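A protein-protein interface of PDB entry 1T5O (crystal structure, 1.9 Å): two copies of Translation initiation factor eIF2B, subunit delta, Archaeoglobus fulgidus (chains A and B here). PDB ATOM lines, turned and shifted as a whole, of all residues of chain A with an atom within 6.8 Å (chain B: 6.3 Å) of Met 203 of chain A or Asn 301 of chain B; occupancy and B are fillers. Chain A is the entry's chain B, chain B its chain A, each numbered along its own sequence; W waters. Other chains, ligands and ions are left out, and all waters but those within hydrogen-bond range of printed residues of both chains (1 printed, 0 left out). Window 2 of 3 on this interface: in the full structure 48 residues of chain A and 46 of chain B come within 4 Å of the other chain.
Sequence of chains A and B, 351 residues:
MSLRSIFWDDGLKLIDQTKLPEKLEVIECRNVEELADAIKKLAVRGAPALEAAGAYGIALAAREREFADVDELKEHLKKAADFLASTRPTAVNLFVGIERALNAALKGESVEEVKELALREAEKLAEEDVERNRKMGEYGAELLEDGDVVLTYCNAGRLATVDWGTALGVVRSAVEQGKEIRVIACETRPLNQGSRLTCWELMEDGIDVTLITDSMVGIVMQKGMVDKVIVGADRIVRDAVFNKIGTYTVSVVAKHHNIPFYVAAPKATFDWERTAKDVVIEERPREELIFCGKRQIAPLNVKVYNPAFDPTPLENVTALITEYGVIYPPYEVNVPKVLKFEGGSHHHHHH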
ATOM      1  N   ARG A 172     -10.877  14.408 -15.001  1.00  0.00           N
ATOM      2  CA  ARG A 172     -11.084  14.279 -16.465  1.00  0.00           C
ATOM      3  C   ARG A 172     -12.574  14.160 -16.841  1.00  0.00           C
ATOM      4  O   ARG A 172     -13.029  14.769 -17.814  1.00  0.00           O
ATOM      5  CB  ARG A 172     -10.312  13.060 -17.033  1.00  0.00           C
ATOM      6  CG  ARG A 172      -8.799  13.308 -17.165  1.00  0.00           C
ATOM      7  CD  ARG A 172      -8.005  12.151 -17.805  1.00  0.00           C
ATOM      8  NE  ARG A 172      -6.611  12.567 -17.900  1.00  0.00           N
ATOM      9  CZ  ARG A 172      -5.708  12.378 -16.943  1.00  0.00           C
ATOM     10  NH1 ARG A 172      -6.038  11.735 -15.814  1.00  0.00           N
ATOM     11  NH2 ARG A 172      -4.503  12.930 -17.067  1.00  0.00           N
ATOM     12  N   LEU A 197       4.959  13.150 -12.255  1.00  0.00           N
ATOM     13  CA  LEU A 197       3.883  12.503 -12.994  1.00  0.00           C
ATOM     14  C   LEU A 197       2.544  13.230 -13.082  1.00  0.00           C
ATOM     15  O   LEU A 197       1.981  13.372 -14.170  1.00  0.00           O
ATOM     16  CB  LEU A 197       3.670  11.100 -12.398  1.00  0.00           C
ATOM     17  CG  LEU A 197       4.943  10.284 -12.086  1.00  0.00           C
ATOM     18  CD1 LEU A 197       4.615   8.969 -11.279  1.00  0.00           C
ATOM     19  CD2 LEU A 197       5.626   9.962 -13.397  1.00  0.00           C
ATOM     20  N   THR A 198       2.021  13.674 -11.945  1.00  0.00           N
ATOM     21  CA  THR A 198       0.737  14.354 -11.959  1.00  0.00           C
ATOM     22  C   THR A 198       0.765  15.623 -12.780  1.00  0.00           C
ATOM     23  O   THR A 198      -0.135  15.852 -13.595  1.00  0.00           O
ATOM     24  CB  THR A 198       0.246  14.632 -10.523  1.00  0.00           C
ATOM     25  OG1 THR A 198       0.025  13.385  -9.893  1.00  0.00           O
ATOM     26  CG2 THR A 198      -1.086  15.442 -10.515  1.00  0.00           C
ATOM     27  N   CYS A 199       1.790  16.444 -12.590  1.00  0.00           N
ATOM     28  CA  CYS A 199       1.888  17.681 -13.336  1.00  0.00           C
ATOM     29  C   CYS A 199       2.087  17.383 -14.809  1.00  0.00           C
ATOM     30  O   CYS A 199       1.555  18.084 -15.681  1.00  0.00           O
ATOM     31  CB  CYS A 199       3.048  18.537 -12.828  1.00  0.00           C
ATOM     32  SG  CYS A 199       2.758  19.241 -11.179  1.00  0.00           S
ATOM     33  N   TRP A 200       2.835  16.324 -15.087  1.00  0.00           N
ATOM     34  CA  TRP A 200       3.083  15.977 -16.469  1.00  0.00           C
ATOM     35  C   TRP A 200       1.806  15.572 -17.182  1.00  0.00           C
ATOM     36  O   TRP A 200       1.480  16.136 -18.240  1.00  0.00           O
ATOM     37  CB  TRP A 200       4.120  14.844 -16.596  1.00  0.00           C
ATOM     38  CG  TRP A 200       4.480  14.576 -18.033  1.00  0.00           C
ATOM     39  CD1 TRP A 200       5.425  15.235 -18.786  1.00  0.00           C
ATOM     40  CD2 TRP A 200       3.811  13.673 -18.937  1.00  0.00           C
ATOM     41  NE1 TRP A 200       5.375  14.799 -20.103  1.00  0.00           N
ATOM     42  CE2 TRP A 200       4.394  13.846 -20.217  1.00  0.00           C
ATOM     43  CE3 TRP A 200       2.772  12.742 -18.788  1.00  0.00           C
ATOM     44  CZ2 TRP A 200       3.969  13.121 -21.344  1.00  0.00           C
ATOM     45  CZ3 TRP A 200       2.343  12.018 -19.918  1.00  0.00           C
ATOM     46  CH2 TRP A 200       2.945  12.218 -21.176  1.00  0.00           C
ATOM     47  N   GLU A 201       1.063  14.617 -16.633  1.00  0.00           N
ATOM     48  CA  GLU A 201      -0.123  14.165 -17.352  1.00  0.00           C
ATOM     49  C   GLU A 201      -1.248  15.184 -17.456  1.00  0.00           C
ATOM     50  O   GLU A 201      -1.978  15.203 -18.449  1.00  0.00           O
ATOM     51  CB  GLU A 201      -0.667  12.841 -16.785  1.00  0.00           C
ATOM     52  CG  GLU A 201      -1.150  12.878 -15.362  1.00  0.00           C
ATOM     53  CD  GLU A 201      -1.808  11.581 -14.968  1.00  0.00           C
ATOM     54  OE1 GLU A 201      -3.033  11.446 -15.189  1.00  0.00           O
ATOM     55  OE2 GLU A 201      -1.094  10.692 -14.463  1.00  0.00           O
ATOM     56  N   LEU A 202      -1.394  16.042 -16.457  1.00  0.00           N
ATOM     57  CA  LEU A 202      -2.450  17.046 -16.530  1.00  0.00           C
ATOM     58  C   LEU A 202      -2.035  18.111 -17.561  1.00  0.00           C
ATOM     59  O   LEU A 202      -2.855  18.579 -18.343  1.00  0.00           O
ATOM     60  CB  LEU A 202      -2.692  17.683 -15.146  1.00  0.00           C
ATOM     61  CG  LEU A 202      -3.303  16.776 -14.060  1.00  0.00           C
ATOM     62  CD1 LEU A 202      -3.502  17.578 -12.778  1.00  0.00           C
ATOM     63  CD2 LEU A 202      -4.625  16.199 -14.513  1.00  0.00           C
ATOM     64  N   MET A 203      -0.761  18.493 -17.568  1.00  0.00           N
ATOM     65  CA  MET A 203      -0.325  19.494 -18.538  1.00  0.00           C
ATOM     66  C   MET A 203      -0.430  18.935 -19.947  1.00  0.00           C
ATOM     67  O   MET A 203      -0.810  19.645 -20.870  1.00  0.00           O
ATOM     68  CB  MET A 203       1.114  19.938 -18.260  1.00  0.00           C
ATOM     69  CG  MET A 203       1.220  21.005 -17.161  1.00  0.00           C
ATOM     70  SD  MET A 203       2.911  21.454 -16.774  1.00  0.00           S
ATOM     71  CE  MET A 203       3.228  22.653 -18.072  1.00  0.00           C
ATOM     72  N   GLU A 204      -0.066  17.666 -20.106  1.00  0.00           N
ATOM     73  CA  GLU A 204      -0.131  16.996 -21.395  1.00  0.00           C
ATOM     74  C   GLU A 204      -1.569  17.015 -21.916  1.00  0.00           C
ATOM     75  O   GLU A 204      -1.796  17.171 -23.124  1.00  0.00           O
ATOM     76  CB  GLU A 204       0.345  15.534 -21.253  1.00  0.00           C
ATOM     77  CG  GLU A 204       0.501  14.793 -22.569  1.00  0.00           C
ATOM     78  CD  GLU A 204       1.724  15.247 -23.372  1.00  0.00           C
ATOM     79  OE1 GLU A 204       1.877  14.784 -24.528  1.00  0.00           O
ATOM     80  OE2 GLU A 204       2.534  16.048 -22.855  1.00  0.00           O
ATOM     81  N   ASP A 205      -2.534  16.873 -21.006  1.00  0.00           N
ATOM     82  CA  ASP A 205      -3.941  16.843 -21.361  1.00  0.00           C
ATOM     83  C   ASP A 205      -4.682  18.193 -21.333  1.00  0.00           C
ATOM     84  O   ASP A 205      -5.904  18.243 -21.488  1.00  0.00           O
ATOM     85  CB  ASP A 205      -4.686  15.845 -20.459  1.00  0.00           C
ATOM     86  CG  ASP A 205      -4.214  14.403 -20.645  1.00  0.00           C
ATOM     87  OD1 ASP A 205      -3.481  14.135 -21.624  1.00  0.00           O
ATOM     88  OD2 ASP A 205      -4.578  13.533 -19.812  1.00  0.00           O
ATOM     89  N   GLY A 206      -3.960  19.281 -21.117  1.00  0.00           N
ATOM     90  CA  GLY A 206      -4.604  20.583 -21.104  1.00  0.00           C
ATOM     91  C   GLY A 206      -5.357  20.965 -19.836  1.00  0.00           C
ATOM     92  O   GLY A 206      -6.158  21.890 -19.863  1.00  0.00           O
ATOM     93  N   ILE A 207      -5.120  20.271 -18.723  1.00  0.00           N
ATOM     94  CA  ILE A 207      -5.815  20.603 -17.473  1.00  0.00           C
ATOM     95  C   ILE A 207      -4.917  21.513 -16.618  1.00  0.00           C
ATOM     96  O   ILE A 207      -3.766  21.175 -16.363  1.00  0.00           O
ATOM     97  CB  ILE A 207      -6.192  19.295 -16.715  1.00  0.00           C
ATOM     98  CG1 ILE A 207      -7.234  18.522 -17.544  1.00  0.00           C
ATOM     99  CG2 ILE A 207      -6.747  19.603 -15.325  1.00  0.00           C
ATOM    100  CD1 ILE A 207      -7.532  17.064 -17.056  1.00  0.00           C
ATOM    101  N   ASP A 208      -5.420  22.675 -16.205  1.00  0.00           N
ATOM    102  CA  ASP A 208      -4.629  23.610 -15.388  1.00  0.00           C
ATOM    103  C   ASP A 208      -4.133  22.944 -14.112  1.00  0.00           C
ATOM    104  O   ASP A 208      -4.918  22.316 -13.381  1.00  0.00           O
ATOM    105  CB  ASP A 208      -5.453  24.834 -14.944  1.00  0.00           C
ATOM    106  CG  ASP A 208      -5.717  25.808 -16.058  1.00  0.00           C
ATOM    107  OD1 ASP A 208      -5.332  25.511 -17.206  1.00  0.00           O
ATOM    108  OD2 ASP A 208      -6.323  26.876 -15.778  1.00  0.00           O
ATOM    109  N   VAL A 209      -2.850  23.109 -13.820  1.00  0.00           N
ATOM    110  CA  VAL A 209      -2.294  22.518 -12.620  1.00  0.00           C
ATOM    111  C   VAL A 209      -1.201  23.428 -12.075  1.00  0.00           C
ATOM    112  O   VAL A 209      -0.376  23.946 -12.831  1.00  0.00           O
ATOM    113  CB  VAL A 209      -1.724  21.079 -12.900  1.00  0.00           C
ATOM    114  CG1 VAL A 209      -0.545  21.145 -13.881  1.00  0.00           C
ATOM    115  CG2 VAL A 209      -1.253  20.415 -11.587  1.00  0.00           C
ATOM    116  N   ARG B 286      10.509  29.983  -8.627  1.00  0.00           N
ATOM    117  CA  ARG B 286       9.799  28.788  -9.054  1.00  0.00           C
ATOM    118  C   ARG B 286      10.737  27.606  -9.336  1.00  0.00           C
ATOM    119  O   ARG B 286      10.317  26.441  -9.275  1.00  0.00           O
ATOM    120  CB  ARG B 286       8.942  29.099 -10.293  1.00  0.00           C
ATOM    121  CG  ARG B 286       9.722  29.589 -11.521  1.00  0.00           C
ATOM    122  CD  ARG B 286       8.778  29.948 -12.658  1.00  0.00           C
ATOM    123  NE  ARG B 286       8.070  28.790 -13.213  1.00  0.00           N
ATOM    124  CZ  ARG B 286       8.576  27.973 -14.134  1.00  0.00           C
ATOM    125  NH1 ARG B 286       9.800  28.178 -14.610  1.00  0.00           N
ATOM    126  NH2 ARG B 286       7.847  26.970 -14.606  1.00  0.00           N
ATOM    127  N   ILE B 290      11.180  22.888  -9.430  1.00  0.00           N
ATOM    128  CA  ILE B 290      11.344  22.267 -10.741  1.00  0.00           C
ATOM    129  C   ILE B 290      12.599  21.403 -10.872  1.00  0.00           C
ATOM    130  O   ILE B 290      12.619  20.425 -11.607  1.00  0.00           O
ATOM    131  CB  ILE B 290      11.295  23.391 -11.847  1.00  0.00           C
ATOM    132  CG1 ILE B 290       9.882  24.002 -11.860  1.00  0.00           C
ATOM    133  CG2 ILE B 290      11.619  22.821 -13.248  1.00  0.00           C
ATOM    134  CD1 ILE B 290       9.705  25.210 -12.774  1.00  0.00           C
ATOM    135  N   ALA B 298      10.046  18.281 -12.241  1.00  0.00           N
ATOM    136  CA  ALA B 298       8.738  18.747 -12.682  1.00  0.00           C
ATOM    137  C   ALA B 298       8.823  19.246 -14.122  1.00  0.00           C
ATOM    138  O   ALA B 298       9.913  19.514 -14.618  1.00  0.00           O
ATOM    139  CB  ALA B 298       8.263  19.892 -11.776  1.00  0.00           C
ATOM    140  N   PRO B 299       7.678  19.359 -14.817  1.00  0.00           N
ATOM    141  CA  PRO B 299       7.746  19.858 -16.197  1.00  0.00           C
ATOM    142  C   PRO B 299       8.322  21.271 -16.104  1.00  0.00           C
ATOM    143  O   PRO B 299       7.986  22.019 -15.186  1.00  0.00           O
ATOM    144  CB  PRO B 299       6.287  19.858 -16.643  1.00  0.00           C
ATOM    145  CG  PRO B 299       5.684  18.724 -15.845  1.00  0.00           C
ATOM    146  CD  PRO B 299       6.317  18.912 -14.478  1.00  0.00           C
ATOM    147  N   LEU B 300       9.183  21.636 -17.054  1.00  0.00           N
ATOM    148  CA  LEU B 300       9.840  22.947 -17.039  1.00  0.00           C
ATOM    149  C   LEU B 300       8.927  24.155 -16.962  1.00  0.00           C
ATOM    150  O   LEU B 300       9.270  25.133 -16.306  1.00  0.00           O
ATOM    151  CB  LEU B 300      10.751  23.107 -18.261  1.00  0.00           C
ATOM    152  CG  LEU B 300      11.887  22.097 -18.382  1.00  0.00           C
ATOM    153  CD1 LEU B 300      12.655  22.366 -19.689  1.00  0.00           C
ATOM    154  CD2 LEU B 300      12.809  22.214 -17.171  1.00  0.00           C
ATOM    155  N   ASN B 301       7.778  24.093 -17.621  1.00  0.00           N
ATOM    156  CA  ASN B 301       6.853  25.223 -17.637  1.00  0.00           C
ATOM    157  C   ASN B 301       5.671  25.103 -16.703  1.00  0.00           C
ATOM    158  O   ASN B 301       4.682  25.807 -16.858  1.00  0.00           O
ATOM    159  CB  ASN B 301       6.334  25.449 -19.052  1.00  0.00           C
ATOM    160  CG  ASN B 301       7.447  25.715 -20.028  1.00  0.00           C
ATOM    161  OD1 ASN B 301       8.482  26.296 -19.673  1.00  0.00           O
ATOM    162  ND2 ASN B 301       7.243  25.309 -21.278  1.00  0.00           N
ATOM    163  N   VAL B 302       5.764  24.227 -15.718  1.00  0.00           N
ATOM    164  CA  VAL B 302       4.655  24.076 -14.791  1.00  0.00           C
ATOM    165  C   VAL B 302       4.517  25.349 -13.950  1.00  0.00           C
ATOM    166  O   VAL B 302       5.507  26.007 -13.624  1.00  0.00           O
ATOM    167  CB  VAL B 302       4.877  22.858 -13.841  1.00  0.00           C
ATOM    168  CG1 VAL B 302       5.994  23.172 -12.837  1.00  0.00           C
ATOM    169  CG2 VAL B 302       3.570  22.493 -13.139  1.00  0.00           C
ATOM    170  N   LYS B 303       3.274  25.708 -13.650  1.00  0.00           N
ATOM    171  CA  LYS B 303       2.969  26.848 -12.795  1.00  0.00           C
ATOM    172  C   LYS B 303       3.294  26.421 -11.356  1.00  0.00           C
ATOM    173  O   LYS B 303       2.915  25.335 -10.920  1.00  0.00           O
ATOM    174  CB  LYS B 303       1.490  27.194 -12.897  1.00  0.00           C
ATOM    175  CG  LYS B 303       1.100  28.371 -12.028  1.00  0.00           C
ATOM    176  CD  LYS B 303      -0.309  28.832 -12.340  1.00  0.00           C
ATOM    177  CE  LYS B 303      -0.530  30.226 -11.785  1.00  0.00           C
ATOM    178  NZ  LYS B 303      -0.160  30.284 -10.355  1.00  0.00           N
HETATM  179  O   HOH W   1       1.010  24.197 -14.975  1.00  0.00           O
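No position is printed for both chains. Of the 7 pairs that touch across the chains among the printed residues, none has its exchanged pair printed and touching as well.
Met 203 of chain A touches just these residues of chain B: Pro 299, Asn 301 and Val 302. Asn 301 of chain B touches one residue of chain A. Printed residues of chain B within 4 Å of Cys 199 of chain A: Pro 299 (3.7 Å) and Val 302 (3.9 Å). Printed residues of chain B within 4 Å of Val 209 of chain A: Lys 303. Printed residues of chain A within 4 Å of Val 302 of chain B: Cys 199 and Met 203. Of the printed residues of chain A, Pro 299 of chain B touches Cys 199, Trp 200 and Met 203. The nearest residue of chain B that does not touch Met 203 of chain A is Lys 303 of chain B (5.3 Å).
Of the 14 printed residues of chain A, 4 touch a printed residue of chain B. Hydrophobic or aromatic side chains of chain A within 4 Å of the printed part of chain B: Met 203. Of the 8 printed residues of chain B, 4 touch a printed residue of chain A. Printed residues of chain B that touch a printed residue of chain A: Pro 299, Asn 301, Val 302 and Lys 303. Hydrophobic or aromatic side chains of chain B within 4 Å of the printed part of chain A: Pro 299 and Val 302. Among the printed residues, no Asp or Glu carboxylate lies within 4 Å of a Lys or Arg side-chain nitrogen of the other chain.
The guanidinium group (NH2) of Arg 286 of chain B is in hydrogen-bond range of the backbone carbonyl oxygen (O) of Val 302 of chain B, 2.7 Å away.
Cys 199 of chain A touches Pro 299 of chain B (CB to CD, 3.7 Å). Cys 199 of chain A touches Val 302 of chain B. CG of Pro 299 of chain B touches N of Trp 200 of chain A (3.8 Å). Met 203 of chain A touches Pro 299 of chain B (SD to CB, 3.7 Å). Asn 301 of chain B touches Met 203 of chain A. Met 203 of chain A touches Val 302 of chain B. Val 209 of chain A touches Lys 303 of chain B.
Water W1 lies within hydrogen-bond range of the backbone carbonyl oxygen of Val 209 of chain A, the backbone NH of Lys 303 of chain B and the side-chain sulfur of Met 203 of chain A.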
